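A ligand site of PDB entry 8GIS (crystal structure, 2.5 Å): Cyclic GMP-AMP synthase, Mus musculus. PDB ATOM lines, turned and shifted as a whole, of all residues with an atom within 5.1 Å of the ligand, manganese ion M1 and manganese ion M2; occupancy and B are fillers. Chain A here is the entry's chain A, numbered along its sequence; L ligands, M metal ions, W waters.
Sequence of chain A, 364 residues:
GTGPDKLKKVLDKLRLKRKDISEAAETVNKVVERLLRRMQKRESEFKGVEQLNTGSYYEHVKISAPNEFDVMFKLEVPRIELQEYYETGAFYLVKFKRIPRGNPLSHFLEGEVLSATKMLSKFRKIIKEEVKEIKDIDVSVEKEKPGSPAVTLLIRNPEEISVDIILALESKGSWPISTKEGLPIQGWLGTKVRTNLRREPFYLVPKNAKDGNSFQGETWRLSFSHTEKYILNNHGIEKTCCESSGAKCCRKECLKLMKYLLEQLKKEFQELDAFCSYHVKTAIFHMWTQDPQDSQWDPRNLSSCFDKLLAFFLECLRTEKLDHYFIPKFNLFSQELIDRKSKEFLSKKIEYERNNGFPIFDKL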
ATOM      1  N   GLY A  55      10.202  -3.785 -10.137  1.00  0.00           N
ATOM      2  CA  GLY A  55       8.824  -4.124 -10.444  1.00  0.00           C
ATOM      3  C   GLY A  55       8.000  -2.907 -10.832  1.00  0.00           C
ATOM      4  O   GLY A  55       8.486  -1.782 -10.934  1.00  0.00           O
ATOM      5  N   SER A  56       6.705  -3.167 -11.031  1.00  0.00           N
ATOM      6  CA  SER A  56       5.874  -2.228 -11.774  1.00  0.00           C
ATOM      7  C   SER A  56       5.785  -0.884 -11.062  1.00  0.00           C
ATOM      8  O   SER A  56       5.749   0.159 -11.728  1.00  0.00           O
ATOM      9  CB  SER A  56       4.469  -2.796 -12.002  1.00  0.00           C
ATOM     10  OG  SER A  56       3.785  -3.116 -10.796  1.00  0.00           O
ATOM     11  N   TYR A  57       5.755  -0.891  -9.729  1.00  0.00           N
ATOM     12  CA  TYR A  57       5.546   0.367  -9.031  1.00  0.00           C
ATOM     13  C   TYR A  57       6.701   1.334  -9.259  1.00  0.00           C
ATOM     14  O   TYR A  57       6.491   2.541  -9.367  1.00  0.00           O
ATOM     15  CB  TYR A  57       5.341   0.111  -7.541  1.00  0.00           C
ATOM     16  CG  TYR A  57       5.311   1.383  -6.726  1.00  0.00           C
ATOM     17  CD1 TYR A  57       4.132   2.143  -6.630  1.00  0.00           C
ATOM     18  CD2 TYR A  57       6.452   1.859  -6.080  1.00  0.00           C
ATOM     19  CE1 TYR A  57       4.102   3.330  -5.905  1.00  0.00           C
ATOM     20  CE2 TYR A  57       6.426   3.045  -5.347  1.00  0.00           C
ATOM     21  CZ  TYR A  57       5.233   3.766  -5.262  1.00  0.00           C
ATOM     22  OH  TYR A  57       5.201   4.934  -4.540  1.00  0.00           O
ATOM     23  N   GLU A  59       8.715   1.077 -11.922  1.00  0.00           N
ATOM     24  CA  GLU A  59       8.748   1.385 -13.340  1.00  0.00           C
ATOM     25  C   GLU A  59       7.610   2.329 -13.740  1.00  0.00           C
ATOM     26  O   GLU A  59       7.551   2.752 -14.892  1.00  0.00           O
ATOM     27  CB  GLU A  59       8.691   0.087 -14.165  1.00  0.00           C
ATOM     28  CG  GLU A  59       9.866  -0.897 -13.882  1.00  0.00           C
ATOM     29  CD  GLU A  59       9.496  -2.365 -14.191  1.00  0.00           C
ATOM     30  OE1 GLU A  59       8.287  -2.714 -14.150  1.00  0.00           O
ATOM     31  OE2 GLU A  59      10.415  -3.189 -14.446  1.00  0.00           O
ATOM     32  N   VAL A  61       4.461   1.472 -13.945  1.00  0.00           N
ATOM     33  CA  VAL A  61       3.410   0.791 -14.703  1.00  0.00           C
ATOM     34  C   VAL A  61       2.461  -0.004 -13.799  1.00  0.00           C
ATOM     35  O   VAL A  61       1.678  -0.823 -14.299  1.00  0.00           O
ATOM     36  CB  VAL A  61       4.001  -0.082 -15.831  1.00  0.00           C
ATOM     37  CG1 VAL A  61       4.596   0.818 -16.908  1.00  0.00           C
ATOM     38  CG2 VAL A  61       5.052  -1.037 -15.306  1.00  0.00           C
ATOM     39  N   LYS A  62       2.535   0.211 -12.475  1.00  0.00           N
ATOM     40  CA  LYS A  62       1.555  -0.333 -11.547  1.00  0.00           C
ATOM     41  C   LYS A  62       0.178   0.250 -11.832  1.00  0.00           C
ATOM     42  O   LYS A  62       0.026   1.470 -11.903  1.00  0.00           O
ATOM     43  CB  LYS A  62       1.970   0.015 -10.113  1.00  0.00           C
ATOM     44  CG  LYS A  62       1.069  -0.572  -9.028  1.00  0.00           C
ATOM     45  CD  LYS A  62       1.375  -2.044  -8.879  1.00  0.00           C
ATOM     46  CE  LYS A  62       0.401  -2.729  -7.961  1.00  0.00           C
ATOM     47  NZ  LYS A  62      -0.900  -3.017  -8.609  1.00  0.00           N
ATOM     48  N   GLU A  68       0.991  -3.414  -4.331  1.00  0.00           N
ATOM     49  CA  GLU A  68       1.993  -4.479  -4.449  1.00  0.00           C
ATOM     50  C   GLU A  68       3.331  -3.866  -4.832  1.00  0.00           C
ATOM     51  O   GLU A  68       3.414  -3.166  -5.849  1.00  0.00           O
ATOM     52  CB  GLU A  68       1.573  -5.538  -5.462  1.00  0.00           C
ATOM     53  CG  GLU A  68       2.197  -6.908  -5.207  1.00  0.00           C
ATOM     54  CD  GLU A  68       3.494  -7.111  -5.998  1.00  0.00           C
ATOM     55  OE1 GLU A  68       3.859  -6.197  -6.742  1.00  0.00           O
ATOM     56  OE2 GLU A  68       4.143  -8.160  -5.885  1.00  0.00           O
ATOM     57  N   PHE A  69       4.360  -4.161  -4.022  1.00  0.00           N
ATOM     58  CA  PHE A  69       5.699  -3.590  -4.124  1.00  0.00           C
ATOM     59  C   PHE A  69       6.709  -4.732  -4.166  1.00  0.00           C
ATOM     60  O   PHE A  69       6.553  -5.711  -3.437  1.00  0.00           O
ATOM     61  CB  PHE A  69       6.044  -2.670  -2.911  1.00  0.00           C
ATOM     62  CG  PHE A  69       5.154  -1.463  -2.800  1.00  0.00           C
ATOM     63  CD1 PHE A  69       3.840  -1.578  -2.365  1.00  0.00           C
ATOM     64  CD2 PHE A  69       5.625  -0.208  -3.155  1.00  0.00           C
ATOM     65  CE1 PHE A  69       3.006  -0.452  -2.271  1.00  0.00           C
ATOM     66  CE2 PHE A  69       4.794   0.911  -3.076  1.00  0.00           C
ATOM     67  CZ  PHE A  69       3.485   0.784  -2.635  1.00  0.00           C
ATOM     68  N   ASP A  70       7.715  -4.610  -5.017  1.00  0.00           N
ATOM     69  CA  ASP A  70       8.758  -5.623  -5.101  1.00  0.00           C
ATOM     70  C   ASP A  70      10.095  -5.006  -4.746  1.00  0.00           C
ATOM     71  O   ASP A  70      10.448  -3.942  -5.259  1.00  0.00           O
ATOM     72  CB  ASP A  70       8.824  -6.225  -6.500  1.00  0.00           C
ATOM     73  CG  ASP A  70       7.489  -6.746  -6.933  1.00  0.00           C
ATOM     74  OD1 ASP A  70       7.083  -7.823  -6.450  1.00  0.00           O
ATOM     75  OD2 ASP A  70       6.837  -6.063  -7.748  1.00  0.00           O
ATOM     76  N   ASP A 164       6.877  -7.978  -1.727  1.00  0.00           N
ATOM     77  CA  ASP A 164       7.738  -9.125  -1.988  1.00  0.00           C
ATOM     78  C   ASP A 164       9.181  -8.749  -1.668  1.00  0.00           C
ATOM     79  O   ASP A 164       9.765  -7.877  -2.332  1.00  0.00           O
ATOM     80  CB  ASP A 164       7.603  -9.559  -3.440  1.00  0.00           C
ATOM     81  CG  ASP A 164       6.312 -10.310  -3.684  1.00  0.00           C
ATOM     82  OD1 ASP A 164       5.810 -10.946  -2.722  1.00  0.00           O
ATOM     83  OD2 ASP A 164       5.809 -10.263  -4.823  1.00  0.00           O
ATOM     84  N   ARG A 221      17.809 -19.068 -10.074  1.00  0.00           N
ATOM     85  CA  ARG A 221      17.246 -18.551 -11.318  1.00  0.00           C
ATOM     86  C   ARG A 221      17.791 -17.155 -11.571  1.00  0.00           C
ATOM     87  O   ARG A 221      17.880 -16.334 -10.649  1.00  0.00           O
ATOM     88  CB  ARG A 221      15.693 -18.540 -11.247  1.00  0.00           C
ATOM     89  CG  ARG A 221      14.950 -18.238 -12.565  1.00  0.00           C
ATOM     90  CD  ARG A 221      13.554 -17.661 -12.332  1.00  0.00           C
ATOM     91  NE  ARG A 221      13.607 -16.204 -12.400  1.00  0.00           N
ATOM     92  CZ  ARG A 221      12.962 -15.384 -11.574  1.00  0.00           C
ATOM     93  NH1 ARG A 221      12.096 -15.834 -10.677  1.00  0.00           N
ATOM     94  NH2 ARG A 221      13.215 -14.075 -11.645  1.00  0.00           N
ATOM     95  N   LEU A 222      18.178 -16.878 -12.824  1.00  0.00           N
ATOM     96  CA  LEU A 222      18.669 -15.556 -13.214  1.00  0.00           C
ATOM     97  C   LEU A 222      17.575 -14.495 -13.111  1.00  0.00           C
ATOM     98  O   LEU A 222      16.419 -14.737 -13.481  1.00  0.00           O
ATOM     99  CB  LEU A 222      19.210 -15.567 -14.639  1.00  0.00           C
ATOM    100  CG  LEU A 222      20.618 -16.098 -14.846  1.00  0.00           C
ATOM    101  CD1 LEU A 222      20.906 -16.285 -16.325  1.00  0.00           C
ATOM    102  CD2 LEU A 222      21.609 -15.116 -14.217  1.00  0.00           C
ATOM    103  N   PHE A 224      16.828 -10.238 -13.966  1.00  0.00           N
ATOM    104  CA  PHE A 224      17.213  -9.026 -14.673  1.00  0.00           C
ATOM    105  C   PHE A 224      16.244  -7.907 -14.360  1.00  0.00           C
ATOM    106  O   PHE A 224      16.026  -7.037 -15.210  1.00  0.00           O
ATOM    107  CB  PHE A 224      17.285  -9.252 -16.179  1.00  0.00           C
ATOM    108  CG  PHE A 224      18.355 -10.227 -16.574  1.00  0.00           C
ATOM    109  CD1 PHE A 224      19.675  -9.833 -16.544  1.00  0.00           C
ATOM    110  CD2 PHE A 224      18.040 -11.533 -16.885  1.00  0.00           C
ATOM    111  CE1 PHE A 224      20.678 -10.722 -16.843  1.00  0.00           C
ATOM    112  CE2 PHE A 224      19.050 -12.437 -17.215  1.00  0.00           C
ATOM    113  CZ  PHE A 224      20.356 -12.033 -17.186  1.00  0.00           C
ATOM    114  N   SER A 225      15.647  -7.933 -13.161  1.00  0.00           N
ATOM    115  CA  SER A 225      14.697  -6.886 -12.791  1.00  0.00           C
ATOM    116  C   SER A 225      15.323  -5.515 -12.920  1.00  0.00           C
ATOM    117  O   SER A 225      14.655  -4.570 -13.344  1.00  0.00           O
ATOM    118  CB  SER A 225      14.193  -7.088 -11.375  1.00  0.00           C
ATOM    119  OG  SER A 225      13.318  -8.189 -11.343  1.00  0.00           O
ATOM    120  N   GLU A 228      15.405  -4.505 -16.601  1.00  0.00           N
ATOM    121  CA  GLU A 228      14.048  -4.172 -17.023  1.00  0.00           C
ATOM    122  C   GLU A 228      13.630  -2.804 -16.493  1.00  0.00           C
ATOM    123  O   GLU A 228      12.919  -2.071 -17.187  1.00  0.00           O
ATOM    124  CB  GLU A 228      13.087  -5.270 -16.561  1.00  0.00           C
ATOM    125  CG  GLU A 228      13.433  -6.658 -17.132  1.00  0.00           C
ATOM    126  CD  GLU A 228      12.829  -7.800 -16.330  1.00  0.00           C
ATOM    127  OE1 GLU A 228      11.987  -7.546 -15.446  1.00  0.00           O
ATOM    128  OE2 GLU A 228      13.167  -8.981 -16.601  1.00  0.00           O
ATOM    129  N   LYS A 259      -1.542  -5.382 -19.140  1.00  0.00           N
ATOM    130  CA  LYS A 259      -1.514  -5.877 -17.765  1.00  0.00           C
ATOM    131  C   LYS A 259      -2.929  -6.012 -17.209  1.00  0.00           C
ATOM    132  O   LYS A 259      -3.253  -7.014 -16.546  1.00  0.00           O
ATOM    133  CB  LYS A 259      -0.721  -4.929 -16.870  1.00  0.00           C
ATOM    134  CG  LYS A 259       0.791  -5.097 -16.972  1.00  0.00           C
ATOM    135  CD  LYS A 259       1.495  -3.860 -16.407  1.00  0.00           C
ATOM    136  CE  LYS A 259       1.183  -3.742 -14.939  1.00  0.00           C
ATOM    137  NZ  LYS A 259       2.033  -4.680 -14.147  1.00  0.00           N
ATOM    138  N   GLU A 263      -4.897  -9.195 -15.798  1.00  0.00           N
ATOM    139  CA  GLU A 263      -5.334  -9.121 -14.403  1.00  0.00           C
ATOM    140  C   GLU A 263      -6.843  -9.365 -14.280  1.00  0.00           C
ATOM    141  O   GLU A 263      -7.297 -10.169 -13.456  1.00  0.00           O
ATOM    142  CB  GLU A 263      -4.944  -7.741 -13.848  1.00  0.00           C
ATOM    143  CG  GLU A 263      -4.374  -7.695 -12.455  1.00  0.00           C
ATOM    144  CD  GLU A 263      -3.604  -6.397 -12.172  1.00  0.00           C
ATOM    145  OE1 GLU A 263      -4.013  -5.677 -11.229  1.00  0.00           O
ATOM    146  OE2 GLU A 263      -2.579  -6.091 -12.816  1.00  0.00           O
ATOM    147  N   CYS A 276       1.103 -14.967 -15.872  1.00  0.00           N
ATOM    148  CA  CYS A 276       1.441 -13.909 -14.952  1.00  0.00           C
ATOM    149  C   CYS A 276       1.842 -12.687 -15.764  1.00  0.00           C
ATOM    150  O   CYS A 276       2.165 -12.789 -16.946  1.00  0.00           O
ATOM    151  CB  CYS A 276       2.568 -14.325 -14.001  1.00  0.00           C
ATOM    152  SG  CYS A 276       4.147 -14.618 -14.848  1.00  0.00           S
ATOM    153  N   SER A 277       1.850 -11.532 -15.094  1.00  0.00           N
ATOM    154  CA  SER A 277       2.139 -10.303 -15.820  1.00  0.00           C
ATOM    155  C   SER A 277       3.548 -10.272 -16.418  1.00  0.00           C
ATOM    156  O   SER A 277       3.790  -9.483 -17.339  1.00  0.00           O
ATOM    157  CB  SER A 277       1.907  -9.105 -14.903  1.00  0.00           C
ATOM    158  OG  SER A 277       2.754  -9.169 -13.783  1.00  0.00           O
ATOM    159  N   TYR A 278       4.463 -11.127 -15.965  1.00  0.00           N
ATOM    160  CA  TYR A 278       5.771 -11.154 -16.619  1.00  0.00           C
ATOM    161  C   TYR A 278       5.645 -11.587 -18.076  1.00  0.00           C
ATOM    162  O   TYR A 278       6.470 -11.228 -18.918  1.00  0.00           O
ATOM    163  CB  TYR A 278       6.758 -12.084 -15.890  1.00  0.00           C
ATOM    164  CG  TYR A 278       8.192 -11.887 -16.349  1.00  0.00           C
ATOM    165  CD1 TYR A 278       8.870 -10.705 -16.080  1.00  0.00           C
ATOM    166  CD2 TYR A 278       8.875 -12.854 -17.097  1.00  0.00           C
ATOM    167  CE1 TYR A 278      10.173 -10.491 -16.499  1.00  0.00           C
ATOM    168  CE2 TYR A 278      10.186 -12.649 -17.524  1.00  0.00           C
ATOM    169  CZ  TYR A 278      10.814 -11.452 -17.219  1.00  0.00           C
ATOM    170  OH  TYR A 278      12.121 -11.183 -17.605  1.00  0.00           O
ATOM    171  N   LYS A 281       4.871  -8.530 -19.959  1.00  0.00           N
ATOM    172  CA  LYS A 281       6.040  -7.650 -19.949  1.00  0.00           C
ATOM    173  C   LYS A 281       7.075  -8.131 -20.955  1.00  0.00           C
ATOM    174  O   LYS A 281       7.658  -7.324 -21.705  1.00  0.00           O
ATOM    175  CB  LYS A 281       6.652  -7.597 -18.545  1.00  0.00           C
ATOM    176  CG  LYS A 281       7.680  -6.490 -18.312  1.00  0.00           C
ATOM    177  CD  LYS A 281       8.161  -6.504 -16.862  1.00  0.00           C
ATOM    178  CE  LYS A 281       9.175  -5.393 -16.594  1.00  0.00           C
ATOM    179  NZ  LYS A 281       9.988  -5.663 -15.350  1.00  0.00           N
ATOM    180  N   HIS A 324      12.144 -15.809 -23.398  1.00  0.00           N
ATOM    181  CA  HIS A 324      12.712 -14.902 -22.416  1.00  0.00           C
ATOM    182  C   HIS A 324      13.541 -13.827 -23.112  1.00  0.00           C
ATOM    183  O   HIS A 324      14.332 -14.119 -24.007  1.00  0.00           O
ATOM    184  CB  HIS A 324      13.581 -15.703 -21.440  1.00  0.00           C
ATOM    185  CG  HIS A 324      13.868 -14.986 -20.160  1.00  0.00           C
ATOM    186  ND1 HIS A 324      14.686 -13.882 -20.094  1.00  0.00           N
ATOM    187  CD2 HIS A 324      13.446 -15.223 -18.900  1.00  0.00           C
ATOM    188  CE1 HIS A 324      14.755 -13.459 -18.843  1.00  0.00           C
ATOM    189  NE2 HIS A 324      14.014 -14.261 -18.099  1.00  0.00           N
HETATM  190  P1  LIG L   1       2.624  -6.328 -11.238  1.00  0.00           P
HETATM  191  O1  LIG L   1       1.853  -7.525 -11.679  1.00  0.00           O
HETATM  192  O2  LIG L   1       1.932  -4.948 -11.374  1.00  0.00           O
HETATM  193  O3  LIG L   1       3.083  -6.437  -9.818  1.00  0.00           O
HETATM  194  P2  LIG L   1       5.537  -6.598 -11.875  1.00  0.00           P
HETATM  195  O4  LIG L   1       6.350  -6.519 -13.118  1.00  0.00           O
HETATM  196  O5  LIG L   1       6.079  -5.777 -10.701  1.00  0.00           O
HETATM  197  O6  LIG L   1       4.002  -6.212 -12.063  1.00  0.00           O
HETATM  198  P3  LIG L   1       5.805  -9.073 -10.246  1.00  0.00           P
HETATM  199  O7  LIG L   1       5.189 -10.414 -10.382  1.00  0.00           O
HETATM  200  O8  LIG L   1       5.424  -8.342  -8.991  1.00  0.00           O
HETATM  201  O9  LIG L   1       5.392  -8.136 -11.475  1.00  0.00           O
HETATM  202  O10 LIG L   1       7.356  -9.342 -10.357  1.00  0.00           O
HETATM  203  C1  LIG L   1       8.326  -8.371  -9.934  1.00  0.00           C
HETATM  204  C2  LIG L   1       9.491  -8.479 -10.886  1.00  0.00           C
HETATM  205  O11 LIG L   1      10.111  -9.774 -10.758  1.00  0.00           O
HETATM  206  C3  LIG L   1       9.116  -8.382 -12.363  1.00  0.00           C
HETATM  207  O12 LIG L   1       9.014  -7.026 -12.787  1.00  0.00           O
HETATM  208  C4  LIG L   1      10.270  -9.132 -13.044  1.00  0.00           C
HETATM  209  O13 LIG L   1      11.438  -8.348 -13.221  1.00  0.00           O
HETATM  210  C5  LIG L   1      10.552 -10.238 -12.031  1.00  0.00           C
HETATM  211  N1  LIG L   1       9.856 -11.483 -12.338  1.00  0.00           N
HETATM  212  C6  LIG L   1       8.588 -11.853 -11.961  1.00  0.00           C
HETATM  213  N2  LIG L   1       8.216 -13.032 -12.402  1.00  0.00           N
HETATM  214  C7  LIG L   1       9.314 -13.452 -13.147  1.00  0.00           C
HETATM  215  C8  LIG L   1       9.545 -14.632 -13.891  1.00  0.00           C
HETATM  216  N3  LIG L   1       8.670 -15.635 -13.996  1.00  0.00           N
HETATM  217  N4  LIG L   1      10.753 -14.743 -14.510  1.00  0.00           N
HETATM  218  C9  LIG L   1      11.633 -13.752 -14.399  1.00  0.00           C
HETATM  219  N5  LIG L   1      11.510 -12.602 -13.730  1.00  0.00           N
HETATM  220  C10 LIG L   1      10.319 -12.508 -13.126  1.00  0.00           C
HETATM  221 MN    MN M   1       5.608  -9.392  -6.915  1.00  0.00          MN
HETATM  222 MN    MN M   2       4.864  -6.168  -8.613  1.00  0.00          MN
HETATM  223  O   HOH W   1      -0.269  -3.677 -11.348  1.00  0.00           O
HETATM  224  O   HOH W   2       4.671  -3.828  -8.304  1.00  0.00           O
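CA of Gly 55 touches O5 of the ligand (3.2 Å).
Lys 62 touches the ligand.
Tyr 278 touches the ligand (CE2 to C9, 3.6 Å).
Hydrophobic or aromatic side chains that line the ligand: Tyr 278.
Within 4 Å of the ligand: Gly 55, Ser 56, Lys 62, Glu 68, Asp 70, Arg 221, Ser 225, Glu 228, Lys 259, Ser 277, Tyr 278 and Lys 281.
Residues that only touch manganese ion M2: Ser 56 (3.9 Å).
Of the 22 residues printed, 3 come within 4 Å of manganese ion M2.
Along chain A the residues within 4 Å of manganese ion M2 span positions 56 to 70.
The nearest printed residue that does not touch manganese ion M2 is Gly 55 (4.8 Å).
SG of Cys 276 sits close to N of Tyr 278 (3.7 Å).
The backbone NH of Asp 164 is in hydrogen-bond range of the backbone carbonyl oxygen of Phe 69, 2.9 Å away.
O of Ser 56 lies within hydrogen-bond range of N of Lys 62, at 3.3 Å.
OE2 of Glu 59 lies within salt-bridge range of NZ of Lys 281 (2.7 Å).
OE2 of Glu 228 lies within hydrogen-bond range of OH of Tyr 278 (2.6 Å).
The backbone NH (N) of Val 61 sits at hydrogen-bond distance from the backbone carbonyl oxygen (O) of Ser 56, 2.9 Å away.
The side-chain amino group of Lys 281 is in salt-bridge range of the side-chain carboxylate of Glu 228 (2.7 Å).
OE1 of Glu 68 binds manganese ion M2 (2.1 Å).
The side-chain carboxylate (OD2) of Asp 70 is bound to manganese ion M2, at 2.2 Å.
An oxygen (O3) of the ligand binds manganese ion M2, at 2.2 Å.
Manganese ion M2 is bound by O8 of the ligand, 2.3 Å away.
Water W2 is bound to manganese ion M2 (2.4 Å).
Manganese ion M2 is bound by an oxygen (O5) of the ligand (2.4 Å).
Manganese ion M2 has six donor atoms within binding distance.
Manganese ion M1 is bound by OE2 of Glu 68, at 2.2 Å.
OD1 of Asp 70 is bound to manganese ion M1 (2.2 Å).
OD2 of Asp 164 binds manganese ion M1.
Manganese ion M1 is bound by O8 of the ligand (2.3 Å).
Manganese ion M1 has four donor atoms within binding distance.
The nearest printed residue that does not touch manganese ion M1 is Phe 69 (5.2 Å).
O12 of the ligand is in hydrogen-bond range of NZ of Lys 281, at 3.1 Å.
The side-chain amino group (NZ) of Lys 259 lies within salt-bridge range of an oxygen (O2) of the ligand (2.8 Å).
An oxygen (O5) of the ligand lies close to the backbone NH of Ser 56, 2.7 Å away.
The side-chain hydroxyl of Ser 277 is in hydrogen-bond range of an oxygen (O1) of the ligand, 2.8 Å away.
The side-chain hydroxyl (OG) of Ser 56 is in hydrogen-bond range of an oxygen (O2) of the ligand.
The guanidinium group (NH2) of Arg 221 lies within hydrogen-bond range of a nitrogen (N5) of the ligand, 3.1 Å away.
An oxygen (O13) of the ligand sits at hydrogen-bond distance from the side-chain carboxylate of Glu 228 (2.4 Å).
An oxygen (O13) of the ligand is in hydrogen-bond range of the side-chain hydroxyl (OG) of Ser 225 (2.7 Å).
Water W2 lies within hydrogen-bond range of the side-chain hydroxyl (OG) of Ser 56 (2.7 Å), the backbone carbonyl oxygen (O) of Glu 68 (2.8 Å) and the backbone NH (N) of Tyr 57 (3.4 Å).
Water W1 lies within hydrogen-bond range of an oxygen (O2) of the ligand and the side-chain amino group (NZ) of Lys 62.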
